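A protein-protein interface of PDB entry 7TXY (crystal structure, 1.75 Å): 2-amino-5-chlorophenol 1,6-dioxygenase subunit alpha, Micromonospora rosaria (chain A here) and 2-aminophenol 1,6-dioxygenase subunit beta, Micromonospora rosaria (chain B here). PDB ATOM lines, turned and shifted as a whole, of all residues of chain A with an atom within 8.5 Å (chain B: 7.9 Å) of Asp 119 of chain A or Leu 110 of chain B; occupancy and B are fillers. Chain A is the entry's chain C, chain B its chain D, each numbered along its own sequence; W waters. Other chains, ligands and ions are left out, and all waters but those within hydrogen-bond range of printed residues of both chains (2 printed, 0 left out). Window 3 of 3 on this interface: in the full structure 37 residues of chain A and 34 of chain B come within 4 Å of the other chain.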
ATOM      1  N   GLN A  66     -16.512   0.484 -21.570  1.00  0.00           N
ATOM      2  CA  GLN A  66     -17.005  -0.465 -20.578  1.00  0.00           C
ATOM      3  C   GLN A  66     -16.019  -1.623 -20.474  1.00  0.00           C
ATOM      4  O   GLN A  66     -15.899  -2.434 -21.399  1.00  0.00           O
ATOM      5  CB  GLN A  66     -18.395  -0.959 -20.942  1.00  0.00           C
ATOM      6  CG  GLN A  66     -19.008  -1.897 -19.904  1.00  0.00           C
ATOM      7  CD  GLN A  66     -19.008  -1.300 -18.509  1.00  0.00           C
ATOM      8  OE1 GLN A  66     -18.097  -1.535 -17.720  1.00  0.00           O
ATOM      9  NE2 GLN A  66     -20.039  -0.520 -18.197  1.00  0.00           N
ATOM     10  N   ASP A  68     -15.966  -3.642 -17.540  1.00  0.00           N
ATOM     11  CA  ASP A  68     -16.515  -4.692 -16.689  1.00  0.00           C
ATOM     12  C   ASP A  68     -17.032  -5.808 -17.584  1.00  0.00           C
ATOM     13  O   ASP A  68     -17.922  -5.561 -18.404  1.00  0.00           O
ATOM     14  CB  ASP A  68     -17.633  -4.146 -15.814  1.00  0.00           C
ATOM     15  CG  ASP A  68     -18.220  -5.193 -14.879  1.00  0.00           C
ATOM     16  OD1 ASP A  68     -17.933  -6.398 -15.050  1.00  0.00           O
ATOM     17  OD2 ASP A  68     -18.995  -4.809 -13.973  1.00  0.00           O
ATOM     18  N   PRO A  69     -16.502  -7.030 -17.481  1.00  0.00           N
ATOM     19  CA  PRO A  69     -16.916  -8.080 -18.422  1.00  0.00           C
ATOM     20  C   PRO A  69     -18.360  -8.532 -18.265  1.00  0.00           C
ATOM     21  O   PRO A  69     -18.913  -9.089 -19.220  1.00  0.00           O
ATOM     22  CB  PRO A  69     -15.947  -9.240 -18.127  1.00  0.00           C
ATOM     23  CG  PRO A  69     -14.905  -8.712 -17.234  1.00  0.00           C
ATOM     24  CD  PRO A  69     -15.415  -7.468 -16.582  1.00  0.00           C
ATOM     25  N   ASN A  70     -19.000  -8.320 -17.112  1.00  0.00           N
ATOM     26  CA  ASN A  70     -20.337  -8.862 -16.867  1.00  0.00           C
ATOM     27  C   ASN A  70     -21.094  -8.014 -15.852  1.00  0.00           C
ATOM     28  O   ASN A  70     -21.346  -8.440 -14.719  1.00  0.00           O
ATOM     29  CB  ASN A  70     -20.248 -10.317 -16.399  1.00  0.00           C
ATOM     30  CG  ASN A  70     -21.613 -10.995 -16.308  1.00  0.00           C
ATOM     31  OD1 ASN A  70     -21.798 -11.922 -15.526  1.00  0.00           O
ATOM     32  ND2 ASN A  70     -22.566 -10.536 -17.119  1.00  0.00           N
ATOM     33  N   PRO A  71     -21.516  -6.814 -16.246  1.00  0.00           N
ATOM     34  CA  PRO A  71     -22.501  -6.092 -15.428  1.00  0.00           C
ATOM     35  C   PRO A  71     -23.827  -6.839 -15.434  1.00  0.00           C
ATOM     36  O   PRO A  71     -24.301  -7.277 -16.484  1.00  0.00           O
ATOM     37  CB  PRO A  71     -22.617  -4.725 -16.116  1.00  0.00           C
ATOM     38  CG  PRO A  71     -21.438  -4.623 -17.028  1.00  0.00           C
ATOM     39  CD  PRO A  71     -21.072  -6.031 -17.411  1.00  0.00           C
ATOM     40  N   THR A 116     -13.188   1.839 -17.972  1.00  0.00           N
ATOM     41  CA  THR A 116     -14.188   1.957 -16.914  1.00  0.00           C
ATOM     42  C   THR A 116     -14.527   0.572 -16.380  1.00  0.00           C
ATOM     43  O   THR A 116     -15.195  -0.222 -17.061  1.00  0.00           O
ATOM     44  CB  THR A 116     -15.449   2.658 -17.436  1.00  0.00           C
ATOM     45  OG1 THR A 116     -15.097   3.931 -17.997  1.00  0.00           O
ATOM     46  CG2 THR A 116     -16.474   2.862 -16.316  1.00  0.00           C
ATOM     47  N   ARG A 117     -14.091   0.281 -15.153  1.00  0.00           N
ATOM     48  CA  ARG A 117     -14.416  -0.990 -14.505  1.00  0.00           C
ATOM     49  C   ARG A 117     -14.596  -0.730 -13.016  1.00  0.00           C
ATOM     50  O   ARG A 117     -13.614  -0.726 -12.261  1.00  0.00           O
ATOM     51  CB  ARG A 117     -13.330  -2.031 -14.755  1.00  0.00           C
ATOM     52  CG  ARG A 117     -13.672  -3.402 -14.178  1.00  0.00           C
ATOM     53  CD  ARG A 117     -12.641  -4.453 -14.550  1.00  0.00           C
ATOM     54  NE  ARG A 117     -13.054  -5.770 -14.083  1.00  0.00           N
ATOM     55  CZ  ARG A 117     -12.589  -6.919 -14.554  1.00  0.00           C
ATOM     56  NH1 ARG A 117     -11.676  -6.957 -15.509  1.00  0.00           N
ATOM     57  NH2 ARG A 117     -13.062  -8.059 -14.059  1.00  0.00           N
ATOM     58  N   TYR A 118     -15.842  -0.539 -12.589  1.00  0.00           N
ATOM     59  CA  TYR A 118     -16.144  -0.218 -11.203  1.00  0.00           C
ATOM     60  C   TYR A 118     -17.416  -0.925 -10.762  1.00  0.00           C
ATOM     61  O   TYR A 118     -18.408  -0.959 -11.497  1.00  0.00           O
ATOM     62  CB  TYR A 118     -16.318   1.293 -10.999  1.00  0.00           C
ATOM     63  CG  TYR A 118     -15.129   2.113 -11.430  1.00  0.00           C
ATOM     64  CD1 TYR A 118     -14.068   2.347 -10.563  1.00  0.00           C
ATOM     65  CD2 TYR A 118     -15.068   2.660 -12.705  1.00  0.00           C
ATOM     66  CE1 TYR A 118     -12.977   3.102 -10.956  1.00  0.00           C
ATOM     67  CE2 TYR A 118     -13.979   3.416 -13.105  1.00  0.00           C
ATOM     68  CZ  TYR A 118     -12.938   3.631 -12.227  1.00  0.00           C
ATOM     69  OH  TYR A 118     -11.866   4.379 -12.623  1.00  0.00           O
ATOM     70  N   ASP A 119     -17.381  -1.483  -9.556  1.00  0.00           N
ATOM     71  CA  ASP A 119     -18.585  -2.043  -8.964  1.00  0.00           C
ATOM     72  C   ASP A 119     -19.625  -0.945  -8.786  1.00  0.00           C
ATOM     73  O   ASP A 119     -19.311   0.153  -8.308  1.00  0.00           O
ATOM     74  CB  ASP A 119     -18.264  -2.694  -7.621  1.00  0.00           C
ATOM     75  CG  ASP A 119     -17.589  -4.047  -7.774  1.00  0.00           C
ATOM     76  OD1 ASP A 119     -17.392  -4.498  -8.926  1.00  0.00           O
ATOM     77  OD2 ASP A 119     -17.253  -4.660  -6.740  1.00  0.00           O
ATOM     78  N   GLY A 120     -20.860  -1.233  -9.188  1.00  0.00           N
ATOM     79  CA  GLY A 120     -21.940  -0.284  -9.056  1.00  0.00           C
ATOM     80  C   GLY A 120     -22.013   0.777 -10.131  1.00  0.00           C
ATOM     81  O   GLY A 120     -22.863   1.675 -10.035  1.00  0.00           O
ATOM     82  N   PHE A 121     -21.154   0.716 -11.144  1.00  0.00           N
ATOM     83  CA  PHE A 121     -21.223   1.688 -12.225  1.00  0.00           C
ATOM     84  C   PHE A 121     -22.609   1.624 -12.867  1.00  0.00           C
ATOM     85  O   PHE A 121     -23.110   0.524 -13.134  1.00  0.00           O
ATOM     86  CB  PHE A 121     -20.141   1.420 -13.269  1.00  0.00           C
ATOM     87  CG  PHE A 121     -19.954   2.552 -14.238  1.00  0.00           C
ATOM     88  CD1 PHE A 121     -19.208   3.663 -13.887  1.00  0.00           C
ATOM     89  CD2 PHE A 121     -20.534   2.513 -15.492  1.00  0.00           C
ATOM     90  CE1 PHE A 121     -19.042   4.713 -14.776  1.00  0.00           C
ATOM     91  CE2 PHE A 121     -20.373   3.560 -16.383  1.00  0.00           C
ATOM     92  CZ  PHE A 121     -19.630   4.654 -16.027  1.00  0.00           C
ATOM     93  N   PRO A 122     -23.256   2.759 -13.126  1.00  0.00           N
ATOM     94  CA  PRO A 122     -24.628   2.708 -13.656  1.00  0.00           C
ATOM     95  C   PRO A 122     -24.654   2.237 -15.103  1.00  0.00           C
ATOM     96  O   PRO A 122     -23.836   2.648 -15.931  1.00  0.00           O
ATOM     97  CB  PRO A 122     -25.121   4.154 -13.524  1.00  0.00           C
ATOM     98  CG  PRO A 122     -23.882   5.000 -13.431  1.00  0.00           C
ATOM     99  CD  PRO A 122     -22.725   4.136 -13.048  1.00  0.00           C
ATOM    100  N   GLN B  54     -17.689   7.507   3.356  1.00  0.00           N
ATOM    101  CA  GLN B  54     -18.660   6.947   2.428  1.00  0.00           C
ATOM    102  C   GLN B  54     -18.128   6.848   1.005  1.00  0.00           C
ATOM    103  O   GLN B  54     -18.710   6.123   0.189  1.00  0.00           O
ATOM    104  CB  GLN B  54     -19.935   7.793   2.447  1.00  0.00           C
ATOM    105  CG  GLN B  54     -20.672   7.789   3.781  1.00  0.00           C
ATOM    106  CD  GLN B  54     -20.283   8.960   4.672  1.00  0.00           C
ATOM    107  OE1 GLN B  54     -19.189   9.514   4.558  1.00  0.00           O
ATOM    108  NE2 GLN B  54     -21.188   9.342   5.567  1.00  0.00           N
ATOM    109  N   ASN B  55     -17.043   7.549   0.685  1.00  0.00           N
ATOM    110  CA  ASN B  55     -16.510   7.583  -0.670  1.00  0.00           C
ATOM    111  C   ASN B  55     -15.393   6.563  -0.820  1.00  0.00           C
ATOM    112  O   ASN B  55     -14.413   6.588  -0.066  1.00  0.00           O
ATOM    113  CB  ASN B  55     -15.987   8.979  -1.020  1.00  0.00           C
ATOM    114  CG  ASN B  55     -15.967   9.225  -2.511  1.00  0.00           C
ATOM    115  OD1 ASN B  55     -16.778   8.658  -3.254  1.00  0.00           O
ATOM    116  ND2 ASN B  55     -15.044  10.064  -2.963  1.00  0.00           N
ATOM    117  N   GLU B  56     -15.534   5.681  -1.818  1.00  0.00           N
ATOM    118  CA  GLU B  56     -14.533   4.628  -2.002  1.00  0.00           C
ATOM    119  C   GLU B  56     -13.211   5.193  -2.502  1.00  0.00           C
ATOM    120  O   GLU B  56     -12.172   4.959  -1.860  1.00  0.00           O
ATOM    121  CB  GLU B  56     -15.081   3.545  -2.935  1.00  0.00           C
ATOM    122  CG  GLU B  56     -14.398   2.193  -2.785  1.00  0.00           C
ATOM    123  CD  GLU B  56     -14.842   1.194  -3.839  1.00  0.00           C
ATOM    124  OE1 GLU B  56     -16.049   1.159  -4.158  1.00  0.00           O
ATOM    125  OE2 GLU B  56     -13.987   0.442  -4.351  1.00  0.00           O
ATOM    126  N   PRO B  57     -13.161   5.930  -3.611  1.00  0.00           N
ATOM    127  CA  PRO B  57     -11.868   6.440  -4.081  1.00  0.00           C
ATOM    128  C   PRO B  57     -11.243   7.389  -3.067  1.00  0.00           C
ATOM    129  O   PRO B  57     -11.922   7.977  -2.222  1.00  0.00           O
ATOM    130  CB  PRO B  57     -12.212   7.162  -5.392  1.00  0.00           C
ATOM    131  CG  PRO B  57     -13.667   7.437  -5.324  1.00  0.00           C
ATOM    132  CD  PRO B  57     -14.275   6.347  -4.484  1.00  0.00           C
ATOM    133  N   ARG B 108     -31.107   4.521   0.404  1.00  0.00           N
ATOM    134  CA  ARG B 108     -29.779   3.972   0.628  1.00  0.00           C
ATOM    135  C   ARG B 108     -29.295   3.333  -0.665  1.00  0.00           C
ATOM    136  O   ARG B 108     -30.097   2.871  -1.479  1.00  0.00           O
ATOM    137  CB  ARG B 108     -29.746   2.927   1.752  1.00  0.00           C
ATOM    138  CG  ARG B 108     -30.695   3.188   2.907  1.00  0.00           C
ATOM    139  CD  ARG B 108     -30.935   1.923   3.727  1.00  0.00           C
ATOM    140  NE  ARG B 108     -32.321   1.830   4.176  1.00  0.00           N
ATOM    141  CZ  ARG B 108     -33.033   0.711   4.216  1.00  0.00           C
ATOM    142  NH1 ARG B 108     -32.516  -0.454   3.856  1.00  0.00           N
ATOM    143  NH2 ARG B 108     -34.297   0.763   4.627  1.00  0.00           N
ATOM    144  N   GLY B 109     -27.982   3.301  -0.840  1.00  0.00           N
ATOM    145  CA  GLY B 109     -27.402   2.677  -2.010  1.00  0.00           C
ATOM    146  C   GLY B 109     -25.985   3.164  -2.239  1.00  0.00           C
ATOM    147  O   GLY B 109     -25.380   3.794  -1.379  1.00  0.00           O
ATOM    148  N   LEU B 110     -25.475   2.844  -3.426  1.00  0.00           N
ATOM    149  CA  LEU B 110     -24.152   3.258  -3.873  1.00  0.00           C
ATOM    150  C   LEU B 110     -24.318   4.194  -5.063  1.00  0.00           C
ATOM    151  O   LEU B 110     -24.928   3.822  -6.072  1.00  0.00           O
ATOM    152  CB  LEU B 110     -23.300   2.050  -4.255  1.00  0.00           C
ATOM    153  CG  LEU B 110     -21.837   2.334  -4.609  1.00  0.00           C
ATOM    154  CD1 LEU B 110     -21.117   3.036  -3.472  1.00  0.00           C
ATOM    155  CD2 LEU B 110     -21.111   1.044  -4.980  1.00  0.00           C
ATOM    156  N   SER B 111     -23.781   5.404  -4.947  1.00  0.00           N
ATOM    157  CA  SER B 111     -23.904   6.426  -5.982  1.00  0.00           C
ATOM    158  C   SER B 111     -22.555   6.547  -6.683  1.00  0.00           C
ATOM    159  O   SER B 111     -21.558   6.945  -6.066  1.00  0.00           O
ATOM    160  CB  SER B 111     -24.348   7.755  -5.380  1.00  0.00           C
ATOM    161  OG  SER B 111     -24.282   8.809  -6.332  1.00  0.00           O
ATOM    162  N   VAL B 112     -22.520   6.182  -7.961  1.00  0.00           N
ATOM    163  CA  VAL B 112     -21.305   6.230  -8.766  1.00  0.00           C
ATOM    164  C   VAL B 112     -21.472   7.332  -9.805  1.00  0.00           C
ATOM    165  O   VAL B 112     -22.408   7.299 -10.611  1.00  0.00           O
ATOM    166  CB  VAL B 112     -21.012   4.881  -9.436  1.00  0.00           C
ATOM    167  CG1 VAL B 112     -19.787   4.984 -10.342  1.00  0.00           C
ATOM    168  CG2 VAL B 112     -20.812   3.793  -8.392  1.00  0.00           C
ATOM    169  N   GLU B 113     -20.577   8.309  -9.776  1.00  0.00           N
ATOM    170  CA  GLU B 113     -20.550   9.370 -10.780  1.00  0.00           C
ATOM    171  C   GLU B 113     -20.091   8.769 -12.102  1.00  0.00           C
ATOM    172  O   GLU B 113     -18.928   8.355 -12.205  1.00  0.00           O
ATOM    173  CB  GLU B 113     -19.609  10.487 -10.335  1.00  0.00           C
ATOM    174  CG  GLU B 113     -20.080  11.911 -10.636  1.00  0.00           C
ATOM    175  CD  GLU B 113     -19.990  12.274 -12.106  1.00  0.00           C
ATOM    176  OE1 GLU B 113     -19.520  11.442 -12.910  1.00  0.00           O
ATOM    177  OE2 GLU B 113     -20.377  13.407 -12.456  1.00  0.00           O
ATOM    178  N   PRO B 117     -16.121   8.271 -12.185  1.00  0.00           N
ATOM    179  CA  PRO B 117     -16.215   7.132 -11.254  1.00  0.00           C
ATOM    180  C   PRO B 117     -14.951   6.926 -10.448  1.00  0.00           C
ATOM    181  O   PRO B 117     -15.003   6.309  -9.376  1.00  0.00           O
ATOM    182  CB  PRO B 117     -16.499   5.943 -12.182  1.00  0.00           C
ATOM    183  CG  PRO B 117     -15.911   6.340 -13.493  1.00  0.00           C
ATOM    184  CD  PRO B 117     -16.100   7.840 -13.594  1.00  0.00           C
ATOM    185  N   PHE B 120     -15.784   9.544  -7.365  1.00  0.00           N
ATOM    186  CA  PHE B 120     -16.994   9.594  -6.548  1.00  0.00           C
ATOM    187  C   PHE B 120     -17.745   8.274  -6.696  1.00  0.00           C
ATOM    188  O   PHE B 120     -18.398   8.026  -7.717  1.00  0.00           O
ATOM    189  CB  PHE B 120     -17.855  10.784  -6.962  1.00  0.00           C
ATOM    190  CG  PHE B 120     -19.100  10.966  -6.138  1.00  0.00           C
ATOM    191  CD1 PHE B 120     -20.264  10.302  -6.466  1.00  0.00           C
ATOM    192  CD2 PHE B 120     -19.104  11.820  -5.043  1.00  0.00           C
ATOM    193  CE1 PHE B 120     -21.415  10.473  -5.716  1.00  0.00           C
ATOM    194  CE2 PHE B 120     -20.255  11.999  -4.291  1.00  0.00           C
ATOM    195  CZ  PHE B 120     -21.408  11.326  -4.628  1.00  0.00           C
ATOM    196  N   ARG B 121     -17.647   7.437  -5.670  1.00  0.00           N
ATOM    197  CA  ARG B 121     -18.457   6.216  -5.535  1.00  0.00           C
ATOM    198  C   ARG B 121     -18.901   6.219  -4.072  1.00  0.00           C
ATOM    199  O   ARG B 121     -18.169   5.756  -3.193  1.00  0.00           O
ATOM    200  CB  ARG B 121     -17.670   4.976  -5.912  1.00  0.00           C
ATOM    201  CG  ARG B 121     -16.968   5.103  -7.259  1.00  0.00           C
ATOM    202  CD  ARG B 121     -16.552   3.750  -7.820  1.00  0.00           C
ATOM    203  NE  ARG B 121     -15.487   3.134  -7.045  1.00  0.00           N
ATOM    204  CZ  ARG B 121     -14.211   3.491  -7.101  1.00  0.00           C
ATOM    205  NH1 ARG B 121     -13.799   4.470  -7.887  1.00  0.00           N
ATOM    206  NH2 ARG B 121     -13.323   2.844  -6.351  1.00  0.00           N
ATOM    207  N   TYR B 122     -20.086   6.770  -3.825  1.00  0.00           N
ATOM    208  CA  TYR B 122     -20.503   7.214  -2.501  1.00  0.00           C
ATOM    209  C   TYR B 122     -21.618   6.324  -1.974  1.00  0.00           C
ATOM    210  O   TYR B 122     -22.658   6.176  -2.622  1.00  0.00           O
ATOM    211  CB  TYR B 122     -20.973   8.673  -2.558  1.00  0.00           C
ATOM    212  CG  TYR B 122     -21.065   9.360  -1.214  1.00  0.00           C
ATOM    213  CD1 TYR B 122     -22.174   9.188  -0.396  1.00  0.00           C
ATOM    214  CD2 TYR B 122     -20.045  10.192  -0.769  1.00  0.00           C
ATOM    215  CE1 TYR B 122     -22.260   9.820   0.833  1.00  0.00           C
ATOM    216  CE2 TYR B 122     -20.120  10.823   0.458  1.00  0.00           C
ATOM    217  CZ  TYR B 122     -21.233  10.633   1.252  1.00  0.00           C
ATOM    218  OH  TYR B 122     -21.304  11.260   2.476  1.00  0.00           O
ATOM    219  N   ARG B 123     -21.403   5.754  -0.792  1.00  0.00           N
ATOM    220  CA  ARG B 123     -22.390   4.910  -0.125  1.00  0.00           C
ATOM    221  C   ARG B 123     -23.238   5.792   0.781  1.00  0.00           C
ATOM    222  O   ARG B 123     -22.760   6.272   1.815  1.00  0.00           O
ATOM    223  CB  ARG B 123     -21.693   3.804   0.665  1.00  0.00           C
ATOM    224  CG  ARG B 123     -22.607   2.960   1.541  1.00  0.00           C
ATOM    225  CD  ARG B 123     -23.321   1.897   0.733  1.00  0.00           C
ATOM    226  NE  ARG B 123     -22.388   0.972   0.099  1.00  0.00           N
ATOM    227  CZ  ARG B 123     -22.731   0.072  -0.813  1.00  0.00           C
ATOM    228  NH1 ARG B 123     -23.986  -0.066  -1.207  1.00  0.00           N
ATOM    229  NH2 ARG B 123     -21.790  -0.701  -1.347  1.00  0.00           N
ATOM    230  N   TYR B 124     -24.489   6.009   0.401  1.00  0.00           N
ATOM    231  CA  TYR B 124     -25.358   6.945   1.096  1.00  0.00           C
ATOM    232  C   TYR B 124     -26.426   6.215   1.903  1.00  0.00           C
ATOM    233  O   TYR B 124     -26.777   5.067   1.625  1.00  0.00           O
ATOM    234  CB  TYR B 124     -26.025   7.913   0.112  1.00  0.00           C
ATOM    235  CG  TYR B 124     -26.937   7.266  -0.904  1.00  0.00           C
ATOM    236  CD1 TYR B 124     -28.291   7.091  -0.642  1.00  0.00           C
ATOM    237  CD2 TYR B 124     -26.449   6.842  -2.132  1.00  0.00           C
ATOM    238  CE1 TYR B 124     -29.130   6.507  -1.576  1.00  0.00           C
ATOM    239  CE2 TYR B 124     -27.282   6.257  -3.072  1.00  0.00           C
ATOM    240  CZ  TYR B 124     -28.618   6.089  -2.786  1.00  0.00           C
ATOM    241  OH  TYR B 124     -29.444   5.514  -3.720  1.00  0.00           O
ATOM    242  N   ASP B 125     -26.931   6.915   2.917  1.00  0.00           N
ATOM    243  CA  ASP B 125     -27.962   6.408   3.814  1.00  0.00           C
ATOM    244  C   ASP B 125     -28.524   7.582   4.610  1.00  0.00           C
ATOM    245  O   ASP B 125     -27.883   8.060   5.555  1.00  0.00           O
ATOM    246  CB  ASP B 125     -27.391   5.340   4.743  1.00  0.00           C
ATOM    247  CG  ASP B 125     -28.425   4.792   5.716  1.00  0.00           C
ATOM    248  OD1 ASP B 125     -29.552   5.324   5.769  1.00  0.00           O
ATOM    249  OD2 ASP B 125     -28.102   3.820   6.431  1.00  0.00           O
ATOM    250  N   ARG B 156     -32.071   4.771  -7.647  1.00  0.00           N
ATOM    251  CA  ARG B 156     -30.806   5.267  -7.126  1.00  0.00           C
ATOM    252  C   ARG B 156     -30.831   6.788  -7.073  1.00  0.00           C
ATOM    253  O   ARG B 156     -31.201   7.445  -8.053  1.00  0.00           O
ATOM    254  CB  ARG B 156     -29.663   4.769  -8.010  1.00  0.00           C
ATOM    255  CG  ARG B 156     -28.268   5.077  -7.524  1.00  0.00           C
ATOM    256  CD  ARG B 156     -27.249   4.624  -8.570  1.00  0.00           C
ATOM    257  NE  ARG B 156     -26.847   3.233  -8.379  1.00  0.00           N
ATOM    258  CZ  ARG B 156     -26.822   2.306  -9.331  1.00  0.00           C
ATOM    259  NH1 ARG B 156     -27.203   2.571 -10.571  1.00  0.00           N
ATOM    260  NH2 ARG B 156     -26.407   1.078  -9.029  1.00  0.00           N
ATOM    261  N   VAL B 157     -30.452   7.346  -5.921  1.00  0.00           N
ATOM    262  CA  VAL B 157     -30.366   8.796  -5.793  1.00  0.00           C
ATOM    263  C   VAL B 157     -29.165   9.299  -6.585  1.00  0.00           C
ATOM    264  O   VAL B 157     -28.086   8.696  -6.568  1.00  0.00           O
ATOM    265  CB  VAL B 157     -30.271   9.208  -4.316  1.00  0.00           C
ATOM    266  CG1 VAL B 157     -30.234  10.731  -4.194  1.00  0.00           C
ATOM    267  CG2 VAL B 157     -31.444   8.648  -3.532  1.00  0.00           C
ATOM    268  N   ILE B 162     -26.486  13.605  -3.874  1.00  0.00           N
ATOM    269  CA  ILE B 162     -25.641  13.036  -2.826  1.00  0.00           C
ATOM    270  C   ILE B 162     -24.472  13.966  -2.528  1.00  0.00           C
ATOM    271  O   ILE B 162     -24.155  14.246  -1.365  1.00  0.00           O
ATOM    272  CB  ILE B 162     -25.152  11.636  -3.235  1.00  0.00           C
ATOM    273  CG1 ILE B 162     -26.334  10.677  -3.442  1.00  0.00           C
ATOM    274  CG2 ILE B 162     -24.186  11.081  -2.199  1.00  0.00           C
ATOM    275  CD1 ILE B 162     -27.246  10.534  -2.245  1.00  0.00           C
HETATM  276  O   HOH W   1     -17.335   0.761  -6.488  1.00  0.00           O
HETATM  277  O   HOH W   2     -25.032  -0.247 -11.023  1.00  0.00           O
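Asp 119 of chain A touches two residues of chain B. No residue of chain A comes within 4 Å of Gly 109 of chain B. Printed residues of chain B within 4 Å of Gly 120 of chain A: Val 112 (3.4 Å) and Arg 156 (3.7 Å). Of the printed residues of chain A, Arg 156 of chain B touches Gly 120 and Pro 122. Val 157 of chain B touches none of the printed residues of chain A.
The side-chain carboxylate (OE2) of Glu 56 of chain B lies within salt-bridge range of the guanidinium group (NH2) of Arg 121 of chain B, 3.2 Å away. The guanidinium group (NE) of Arg 156 of chain B is in hydrogen-bond range of the backbone carbonyl oxygen (O) of Leu 110 of chain B, 3.1 Å away. NH1 of Arg 121 of chain B sits at hydrogen-bond distance from O of Pro 117 of chain B (2.7 Å). The side-chain amide oxygen (OD1) of Asn 55 of chain B lies within hydrogen-bond range of the backbone NH (N) of Arg 121 of chain B, 2.8 Å away.
Of the 20 printed residues of chain B, 5 touch a printed residue of chain A. Printed residues of chain B that touch a printed residue of chain A: Leu 110, Val 112, Pro 117, Arg 121 and Arg 156. Hydrophobic or aromatic side chains of chain B that line the printed part of chain A: Leu 110, Val 112 and Pro 117. Of the 12 printed residues of chain A, 5 touch a printed residue of chain B. Among the printed residues, no Asp or Glu carboxylate lies within 4 Å of a Lys or Arg side-chain nitrogen of the other chain.
Tyr 118 of chain A touches Pro 117 of chain B. Tyr 118 of chain A touches Arg 121 of chain B (CD1 to NH1, 3.4 Å). CD2 of Leu 110 of chain B touches O of Asp 119 of chain A, 3.9 Å away. Asp 119 of chain A touches Val 112 of chain B (O to CG2, 3.9 Å). CG2 of Val 112 of chain B touches O of Gly 120 of chain A (3.4 Å). NH2 of Arg 156 of chain B touches O of Gly 120 of chain A, 3.7 Å away. CG1 of Val 112 of chain B touches CD1 of Phe 121 of chain A, 3.8 Å away. Pro 117 of chain B touches Phe 121 of chain A. Pro 122 of chain A touches Val 112 of chain B (CG to O, 3.9 Å). CB of Pro 122 of chain A touches NH1 of Arg 156 of chain B (3.9 Å).
Water W1 lies within hydrogen-bond range of the side-chain carboxylate of Glu 56 of chain B (2.7 Å), the backbone carbonyl oxygen of Asp 119 of chain A (2.8 Å) and the guanidinium group of Arg 121 of chain B (3.1 Å). Water W2 lies within hydrogen-bond range of the guanidinium group of Arg 156 of chain B, the backbone carbonyl oxygen of Phe 121 of chain A and the backbone carbonyl oxygen of Gly 120 of chain A.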
